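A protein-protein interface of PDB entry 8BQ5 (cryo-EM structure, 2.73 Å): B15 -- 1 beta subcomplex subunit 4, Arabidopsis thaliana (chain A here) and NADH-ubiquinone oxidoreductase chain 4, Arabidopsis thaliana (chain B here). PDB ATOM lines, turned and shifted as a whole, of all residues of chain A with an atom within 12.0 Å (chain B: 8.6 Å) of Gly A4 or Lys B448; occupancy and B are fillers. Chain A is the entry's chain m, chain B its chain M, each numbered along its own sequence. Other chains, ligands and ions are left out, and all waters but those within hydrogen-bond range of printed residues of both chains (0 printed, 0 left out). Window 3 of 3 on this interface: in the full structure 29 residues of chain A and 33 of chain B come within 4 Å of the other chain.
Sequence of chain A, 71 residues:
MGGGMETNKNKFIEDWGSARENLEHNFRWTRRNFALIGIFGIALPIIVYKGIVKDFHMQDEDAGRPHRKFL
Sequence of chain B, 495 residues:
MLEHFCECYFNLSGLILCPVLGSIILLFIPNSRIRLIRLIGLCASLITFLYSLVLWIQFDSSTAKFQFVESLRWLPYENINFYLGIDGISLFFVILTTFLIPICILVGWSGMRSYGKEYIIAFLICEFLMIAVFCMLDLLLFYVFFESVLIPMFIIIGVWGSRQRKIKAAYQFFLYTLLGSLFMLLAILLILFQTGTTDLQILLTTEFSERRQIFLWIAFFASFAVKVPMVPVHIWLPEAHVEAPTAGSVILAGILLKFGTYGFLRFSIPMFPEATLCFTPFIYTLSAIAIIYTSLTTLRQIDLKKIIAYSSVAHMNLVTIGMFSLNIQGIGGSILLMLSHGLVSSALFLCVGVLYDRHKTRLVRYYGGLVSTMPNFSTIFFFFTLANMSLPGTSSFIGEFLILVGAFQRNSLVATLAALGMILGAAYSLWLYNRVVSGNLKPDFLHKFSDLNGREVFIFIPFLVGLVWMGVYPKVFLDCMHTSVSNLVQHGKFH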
ATOM      1  N   GLY A   2       0.921 -22.336 -21.100  1.00  0.00           N
ATOM      2  CA  GLY A   2       0.025 -21.195 -21.041  1.00  0.00           C
ATOM      3  C   GLY A   2      -0.618 -21.037 -19.678  1.00  0.00           C
ATOM      4  O   GLY A   2      -0.823 -19.921 -19.198  1.00  0.00           O
ATOM      5  N   GLY A   3      -0.934 -22.166 -19.053  1.00  0.00           N
ATOM      6  CA  GLY A   3      -1.529 -22.161 -17.735  1.00  0.00           C
ATOM      7  C   GLY A   3      -1.149 -23.377 -16.919  1.00  0.00           C
ATOM      8  O   GLY A   3      -0.900 -24.453 -17.470  1.00  0.00           O
ATOM      9  N   GLY A   4      -1.099 -23.217 -15.612  1.00  0.00           N
ATOM     10  CA  GLY A   4      -0.781 -24.328 -14.744  1.00  0.00           C
ATOM     11  C   GLY A   4       0.715 -24.461 -14.516  1.00  0.00           C
ATOM     12  O   GLY A   4       1.531 -24.332 -15.439  1.00  0.00           O
ATOM     13  N   MET A   5       1.081 -24.727 -13.263  1.00  0.00           N
ATOM     14  CA  MET A   5       2.473 -24.937 -12.891  1.00  0.00           C
ATOM     15  C   MET A   5       3.008 -26.291 -13.329  1.00  0.00           C
ATOM     16  O   MET A   5       4.229 -26.450 -13.438  1.00  0.00           O
ATOM     17  CB  MET A   5       2.632 -24.812 -11.379  1.00  0.00           C
ATOM     18  CG  MET A   5       3.160 -23.482 -10.920  1.00  0.00           C
ATOM     19  SD  MET A   5       3.318 -23.431  -9.133  1.00  0.00           S
ATOM     20  CE  MET A   5       4.751 -22.383  -8.987  1.00  0.00           C
ATOM     21  N   GLU A   6       2.131 -27.261 -13.572  1.00  0.00           N
ATOM     22  CA  GLU A   6       2.578 -28.610 -13.883  1.00  0.00           C
ATOM     23  C   GLU A   6       3.389 -28.624 -15.172  1.00  0.00           C
ATOM     24  O   GLU A   6       3.120 -27.874 -16.114  1.00  0.00           O
ATOM     25  CB  GLU A   6       1.378 -29.554 -13.990  1.00  0.00           C
ATOM     26  CG  GLU A   6       0.674 -29.783 -12.660  1.00  0.00           C
ATOM     27  CD  GLU A   6      -0.291 -30.951 -12.690  1.00  0.00           C
ATOM     28  OE1 GLU A   6       0.174 -32.109 -12.643  1.00  0.00           O
ATOM     29  OE2 GLU A   6      -1.514 -30.711 -12.745  1.00  0.00           O
ATOM     30  N   THR A   7       4.404 -29.481 -15.198  1.00  0.00           N
ATOM     31  CA  THR A   7       5.291 -29.563 -16.348  1.00  0.00           C
ATOM     32  C   THR A   7       4.534 -30.036 -17.579  1.00  0.00           C
ATOM     33  O   THR A   7       3.578 -30.811 -17.485  1.00  0.00           O
ATOM     34  CB  THR A   7       6.449 -30.515 -16.060  1.00  0.00           C
ATOM     35  OG1 THR A   7       7.135 -30.827 -17.280  1.00  0.00           O
ATOM     36  CG2 THR A   7       5.922 -31.789 -15.463  1.00  0.00           C
ATOM     37  N   ASN A   8       4.963 -29.555 -18.740  1.00  0.00           N
ATOM     38  CA  ASN A   8       4.447 -30.051 -20.009  1.00  0.00           C
ATOM     39  C   ASN A   8       5.175 -31.345 -20.346  1.00  0.00           C
ATOM     40  O   ASN A   8       6.317 -31.323 -20.816  1.00  0.00           O
ATOM     41  CB  ASN A   8       4.618 -28.998 -21.098  1.00  0.00           C
ATOM     42  CG  ASN A   8       4.159 -27.627 -20.647  1.00  0.00           C
ATOM     43  OD1 ASN A   8       4.818 -26.620 -20.902  1.00  0.00           O
ATOM     44  ND2 ASN A   8       3.019 -27.582 -19.965  1.00  0.00           N
ATOM     45  N   LYS A   9       4.507 -32.470 -20.097  1.00  0.00           N
ATOM     46  CA  LYS A   9       5.113 -33.779 -20.287  1.00  0.00           C
ATOM     47  C   LYS A   9       5.566 -33.965 -21.730  1.00  0.00           C
ATOM     48  O   LYS A   9       4.946 -33.455 -22.666  1.00  0.00           O
ATOM     49  CB  LYS A   9       4.114 -34.877 -19.924  1.00  0.00           C
ATOM     50  CG  LYS A   9       4.421 -35.654 -18.659  1.00  0.00           C
ATOM     51  CD  LYS A   9       4.711 -34.768 -17.467  1.00  0.00           C
ATOM     52  CE  LYS A   9       4.542 -35.571 -16.185  1.00  0.00           C
ATOM     53  NZ  LYS A   9       4.496 -34.723 -14.966  1.00  0.00           N
ATOM     54  N   LEU B 355       9.518 -29.356  -4.883  1.00  0.00           N
ATOM     55  CA  LEU B 355       9.529 -29.283  -6.340  1.00  0.00           C
ATOM     56  C   LEU B 355       8.393 -30.094  -6.948  1.00  0.00           C
ATOM     57  O   LEU B 355       7.813 -29.696  -7.964  1.00  0.00           O
ATOM     58  CB  LEU B 355      10.873 -29.776  -6.872  1.00  0.00           C
ATOM     59  CG  LEU B 355      12.021 -28.767  -6.872  1.00  0.00           C
ATOM     60  CD1 LEU B 355      13.086 -29.182  -7.868  1.00  0.00           C
ATOM     61  CD2 LEU B 355      11.518 -27.363  -7.162  1.00  0.00           C
ATOM     62  N   ARG B 358       4.734 -28.426  -6.764  1.00  0.00           N
ATOM     63  CA  ARG B 358       4.458 -27.401  -7.760  1.00  0.00           C
ATOM     64  C   ARG B 358       4.352 -27.970  -9.171  1.00  0.00           C
ATOM     65  O   ARG B 358       3.437 -27.613  -9.917  1.00  0.00           O
ATOM     66  CB  ARG B 358       5.547 -26.322  -7.719  1.00  0.00           C
ATOM     67  CG  ARG B 358       5.623 -25.558  -6.415  1.00  0.00           C
ATOM     68  CD  ARG B 358       7.029 -25.040  -6.156  1.00  0.00           C
ATOM     69  NE  ARG B 358       7.054 -24.002  -5.133  1.00  0.00           N
ATOM     70  CZ  ARG B 358       6.854 -24.217  -3.840  1.00  0.00           C
ATOM     71  NH1 ARG B 358       6.593 -25.427  -3.372  1.00  0.00           N
ATOM     72  NH2 ARG B 358       6.918 -23.193  -2.994  1.00  0.00           N
ATOM     73  N   HIS B 359       5.270 -28.858  -9.550  1.00  0.00           N
ATOM     74  CA  HIS B 359       5.437 -29.226 -10.950  1.00  0.00           C
ATOM     75  C   HIS B 359       5.014 -30.651 -11.271  1.00  0.00           C
ATOM     76  O   HIS B 359       4.856 -30.977 -12.453  1.00  0.00           O
ATOM     77  CB  HIS B 359       6.895 -29.013 -11.362  1.00  0.00           C
ATOM     78  CG  HIS B 359       7.387 -27.627 -11.087  1.00  0.00           C
ATOM     79  ND1 HIS B 359       6.712 -26.506 -11.516  1.00  0.00           N
ATOM     80  CD2 HIS B 359       8.456 -27.180 -10.389  1.00  0.00           C
ATOM     81  CE1 HIS B 359       7.359 -25.426 -11.116  1.00  0.00           C
ATOM     82  NE2 HIS B 359       8.420 -25.807 -10.429  1.00  0.00           N
ATOM     83  N   TYR B 367      13.792 -30.436 -15.061  1.00  0.00           N
ATOM     84  CA  TYR B 367      14.209 -29.277 -14.291  1.00  0.00           C
ATOM     85  C   TYR B 367      15.488 -28.682 -14.875  1.00  0.00           C
ATOM     86  O   TYR B 367      15.974 -29.093 -15.930  1.00  0.00           O
ATOM     87  CB  TYR B 367      14.388 -29.655 -12.823  1.00  0.00           C
ATOM     88  CG  TYR B 367      13.120 -30.127 -12.153  1.00  0.00           C
ATOM     89  CD1 TYR B 367      12.191 -29.218 -11.665  1.00  0.00           C
ATOM     90  CD2 TYR B 367      12.848 -31.481 -12.011  1.00  0.00           C
ATOM     91  CE1 TYR B 367      11.033 -29.642 -11.051  1.00  0.00           C
ATOM     92  CE2 TYR B 367      11.690 -31.914 -11.400  1.00  0.00           C
ATOM     93  CZ  TYR B 367      10.786 -30.991 -10.920  1.00  0.00           C
ATOM     94  OH  TYR B 367       9.630 -31.414 -10.308  1.00  0.00           O
ATOM     95  N   LEU B 370      16.873 -23.584 -11.974  1.00  0.00           N
ATOM     96  CA  LEU B 370      16.003 -23.128 -10.899  1.00  0.00           C
ATOM     97  C   LEU B 370      16.657 -22.081 -10.008  1.00  0.00           C
ATOM     98  O   LEU B 370      15.963 -21.476  -9.184  1.00  0.00           O
ATOM     99  CB  LEU B 370      15.557 -24.320 -10.054  1.00  0.00           C
ATOM    100  CG  LEU B 370      14.501 -25.217 -10.698  1.00  0.00           C
ATOM    101  CD1 LEU B 370      14.122 -26.337  -9.757  1.00  0.00           C
ATOM    102  CD2 LEU B 370      13.279 -24.409 -11.088  1.00  0.00           C
ATOM    103  N   THR B 373      15.053 -18.690 -10.676  1.00  0.00           N
ATOM    104  CA  THR B 373      13.656 -18.520 -10.304  1.00  0.00           C
ATOM    105  C   THR B 373      13.359 -18.900  -8.862  1.00  0.00           C
ATOM    106  O   THR B 373      12.394 -18.380  -8.295  1.00  0.00           O
ATOM    107  CB  THR B 373      12.750 -19.344 -11.230  1.00  0.00           C
ATOM    108  OG1 THR B 373      13.123 -20.725 -11.165  1.00  0.00           O
ATOM    109  CG2 THR B 373      12.875 -18.860 -12.661  1.00  0.00           C
ATOM    110  N   MET B 374      14.154 -19.781  -8.259  1.00  0.00           N
ATOM    111  CA  MET B 374      13.965 -20.203  -6.870  1.00  0.00           C
ATOM    112  C   MET B 374      15.286 -20.116  -6.112  1.00  0.00           C
ATOM    113  O   MET B 374      15.835 -21.133  -5.681  1.00  0.00           O
ATOM    114  CB  MET B 374      13.400 -21.621  -6.814  1.00  0.00           C
ATOM    115  CG  MET B 374      12.161 -21.837  -7.663  1.00  0.00           C
ATOM    116  SD  MET B 374      11.676 -23.569  -7.769  1.00  0.00           S
ATOM    117  CE  MET B 374      11.052 -23.851  -6.116  1.00  0.00           C
ATOM    118  N   LEU B 441      16.951 -22.299 -17.800  1.00  0.00           N
ATOM    119  CA  LEU B 441      15.569 -22.737 -17.748  1.00  0.00           C
ATOM    120  C   LEU B 441      15.172 -23.386 -19.070  1.00  0.00           C
ATOM    121  O   LEU B 441      15.748 -23.115 -20.128  1.00  0.00           O
ATOM    122  CB  LEU B 441      14.640 -21.560 -17.452  1.00  0.00           C
ATOM    123  CG  LEU B 441      14.687 -20.964 -16.046  1.00  0.00           C
ATOM    124  CD1 LEU B 441      14.109 -19.560 -16.055  1.00  0.00           C
ATOM    125  CD2 LEU B 441      13.945 -21.845 -15.057  1.00  0.00           C
ATOM    126  N   LYS B 442      14.166 -24.258 -19.002  1.00  0.00           N
ATOM    127  CA  LYS B 442      13.607 -24.928 -20.172  1.00  0.00           C
ATOM    128  C   LYS B 442      12.125 -24.578 -20.239  1.00  0.00           C
ATOM    129  O   LYS B 442      11.272 -25.332 -19.748  1.00  0.00           O
ATOM    130  CB  LYS B 442      13.842 -26.435 -20.115  1.00  0.00           C
ATOM    131  CG  LYS B 442      15.304 -26.808 -19.947  1.00  0.00           C
ATOM    132  CD  LYS B 442      15.477 -28.130 -19.232  1.00  0.00           C
ATOM    133  CE  LYS B 442      16.943 -28.521 -19.170  1.00  0.00           C
ATOM    134  NZ  LYS B 442      17.141 -29.849 -18.533  1.00  0.00           N
ATOM    135  N   PRO B 443      11.783 -23.434 -20.838  1.00  0.00           N
ATOM    136  CA  PRO B 443      10.389 -22.965 -20.798  1.00  0.00           C
ATOM    137  C   PRO B 443       9.400 -23.865 -21.521  1.00  0.00           C
ATOM    138  O   PRO B 443       8.193 -23.740 -21.281  1.00  0.00           O
ATOM    139  CB  PRO B 443      10.463 -21.576 -21.445  1.00  0.00           C
ATOM    140  CG  PRO B 443      11.745 -21.565 -22.207  1.00  0.00           C
ATOM    141  CD  PRO B 443      12.684 -22.449 -21.456  1.00  0.00           C
ATOM    142  N   PHE B 445       9.193 -27.043 -20.965  1.00  0.00           N
ATOM    143  CA  PHE B 445       8.755 -27.933 -19.898  1.00  0.00           C
ATOM    144  C   PHE B 445       8.154 -27.173 -18.723  1.00  0.00           C
ATOM    145  O   PHE B 445       7.072 -27.523 -18.246  1.00  0.00           O
ATOM    146  CB  PHE B 445       9.925 -28.794 -19.404  1.00  0.00           C
ATOM    147  CG  PHE B 445      10.633 -29.544 -20.493  1.00  0.00           C
ATOM    148  CD1 PHE B 445       9.924 -30.151 -21.513  1.00  0.00           C
ATOM    149  CD2 PHE B 445      12.013 -29.660 -20.480  1.00  0.00           C
ATOM    150  CE1 PHE B 445      10.579 -30.846 -22.510  1.00  0.00           C
ATOM    151  CE2 PHE B 445      12.671 -30.355 -21.471  1.00  0.00           C
ATOM    152  CZ  PHE B 445      11.953 -30.948 -22.487  1.00  0.00           C
ATOM    153  N   LEU B 446       8.842 -26.139 -18.242  1.00  0.00           N
ATOM    154  CA  LEU B 446       8.404 -25.384 -17.078  1.00  0.00           C
ATOM    155  C   LEU B 446       8.618 -23.900 -17.323  1.00  0.00           C
ATOM    156  O   LEU B 446       9.728 -23.476 -17.654  1.00  0.00           O
ATOM    157  CB  LEU B 446       9.160 -25.824 -15.817  1.00  0.00           C
ATOM    158  CG  LEU B 446       8.892 -27.247 -15.330  1.00  0.00           C
ATOM    159  CD1 LEU B 446       9.989 -27.724 -14.397  1.00  0.00           C
ATOM    160  CD2 LEU B 446       7.543 -27.299 -14.642  1.00  0.00           C
ATOM    161  N   HIS B 447       7.554 -23.117 -17.155  1.00  0.00           N
ATOM    162  CA  HIS B 447       7.642 -21.672 -17.309  1.00  0.00           C
ATOM    163  C   HIS B 447       7.009 -20.898 -16.165  1.00  0.00           C
ATOM    164  O   HIS B 447       6.973 -19.667 -16.231  1.00  0.00           O
ATOM    165  CB  HIS B 447       6.993 -21.233 -18.630  1.00  0.00           C
ATOM    166  CG  HIS B 447       5.503 -21.385 -18.653  1.00  0.00           C
ATOM    167  ND1 HIS B 447       4.873 -22.590 -18.431  1.00  0.00           N
ATOM    168  CD2 HIS B 447       4.519 -20.481 -18.871  1.00  0.00           C
ATOM    169  CE1 HIS B 447       3.565 -22.422 -18.510  1.00  0.00           C
ATOM    170  NE2 HIS B 447       3.324 -21.152 -18.778  1.00  0.00           N
ATOM    171  N   LYS B 448       6.524 -21.564 -15.122  1.00  0.00           N
ATOM    172  CA  LYS B 448       5.827 -20.928 -14.014  1.00  0.00           C
ATOM    173  C   LYS B 448       6.409 -21.442 -12.705  1.00  0.00           C
ATOM    174  O   LYS B 448       6.397 -22.651 -12.453  1.00  0.00           O
ATOM    175  CB  LYS B 448       4.331 -21.229 -14.088  1.00  0.00           C
ATOM    176  CG  LYS B 448       3.449 -20.225 -13.394  1.00  0.00           C
ATOM    177  CD  LYS B 448       2.275 -19.848 -14.242  1.00  0.00           C
ATOM    178  CE  LYS B 448       1.073 -20.724 -13.991  1.00  0.00           C
ATOM    179  NZ  LYS B 448       0.590 -20.582 -12.596  1.00  0.00           N
ATOM    180  N   PHE B 449       6.901 -20.532 -11.867  1.00  0.00           N
ATOM    181  CA  PHE B 449       7.647 -20.928 -10.681  1.00  0.00           C
ATOM    182  C   PHE B 449       7.231 -20.104  -9.471  1.00  0.00           C
ATOM    183  O   PHE B 449       6.651 -19.022  -9.598  1.00  0.00           O
ATOM    184  CB  PHE B 449       9.160 -20.797 -10.896  1.00  0.00           C
ATOM    185  CG  PHE B 449       9.660 -21.515 -12.113  1.00  0.00           C
ATOM    186  CD1 PHE B 449       9.700 -20.880 -13.342  1.00  0.00           C
ATOM    187  CD2 PHE B 449      10.074 -22.832 -12.031  1.00  0.00           C
ATOM    188  CE1 PHE B 449      10.154 -21.542 -14.462  1.00  0.00           C
ATOM    189  CE2 PHE B 449      10.527 -23.500 -13.148  1.00  0.00           C
ATOM    190  CZ  PHE B 449      10.568 -22.853 -14.366  1.00  0.00           C
ATOM    191  N   SER B 450       7.524 -20.649  -8.292  1.00  0.00           N
ATOM    192  CA  SER B 450       7.317 -19.972  -7.020  1.00  0.00           C
ATOM    193  C   SER B 450       8.349 -20.478  -6.027  1.00  0.00           C
ATOM    194  O   SER B 450       8.458 -21.688  -5.812  1.00  0.00           O
ATOM    195  CB  SER B 450       5.907 -20.212  -6.473  1.00  0.00           C
ATOM    196  OG  SER B 450       5.623 -19.335  -5.398  1.00  0.00           O
ATOM    197  N   ASP B 451       9.091 -19.556  -5.420  1.00  0.00           N
ATOM    198  CA  ASP B 451      10.041 -19.921  -4.380  1.00  0.00           C
ATOM    199  C   ASP B 451       9.294 -20.367  -3.121  1.00  0.00           C
ATOM    200  O   ASP B 451       8.061 -20.415  -3.076  1.00  0.00           O
ATOM    201  CB  ASP B 451      10.981 -18.754  -4.090  1.00  0.00           C
ATOM    202  CG  ASP B 451      12.383 -19.204  -3.749  1.00  0.00           C
ATOM    203  OD1 ASP B 451      12.551 -20.374  -3.351  1.00  0.00           O
ATOM    204  OD2 ASP B 451      13.320 -18.390  -3.884  1.00  0.00           O
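A ring nitrogen (ND1) of His B359 sits at hydrogen-bond distance from the backbone carbonyl oxygen (O) of Met A5, at 3.1 Å. O of His B359 lies within hydrogen-bond range of N of Thr A7, 3.2 Å away. The side-chain hydroxyl (OG1) of Thr A7 lies close to the backbone carbonyl oxygen (O) of Phe B445 (3.4 Å). The backbone carbonyl oxygen (O) of Phe B445 is in hydrogen-bond range of the backbone NH (N) of Asn A8.
O of Ser B450 sits at hydrogen-bond distance from NE of Arg B358. The guanidinium group (NH2) of Arg B358 lies within hydrogen-bond range of the backbone carbonyl oxygen (O) of Asp B451 (3.0 Å).
Among the printed residues, pairs that only touch across the chains: Gly A2 with His B447, Gly A4 with Lys B448, Met A5 with Arg B358, Met A5 with Leu B446, Met A5 with Lys B448, Met A5 with Phe B449, Met A5 with Ser B450, Glu A6 with Arg B358, Glu A6 with His B359 and Thr A7 with Leu B446.
Lys B448 touches just these residues of chain A: Gly A4 (3.7 Å) and Met A5 (3.7 Å). His B447 touches one residue of chain A. Printed residues of chain B within 4 Å of Thr A7: His B359 (3.2 Å), Phe B445 (3.3 Å) and Leu B446 (3.6 Å). Of the printed residues of chain A, Arg B358 touches Met A5 (3.3 Å) and Glu A6 (3.9 Å). Leu B441 touches none of the printed residues of chain A. The nearest residue of chain A that does not touch Lys B448 is Gly A3 (4.5 Å).
Of the 17 printed residues of chain B, 8 touch a printed residue of chain A. Hydrophobic or aromatic side chains of chain B within 4 Å of the printed part of chain A: His B359, Phe B445, Leu B446 and His B447. Hydrophobic or aromatic side chains of chain A that line the printed part of chain B: Met A5. Among the printed residues, 14 pairs touch across the chains.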
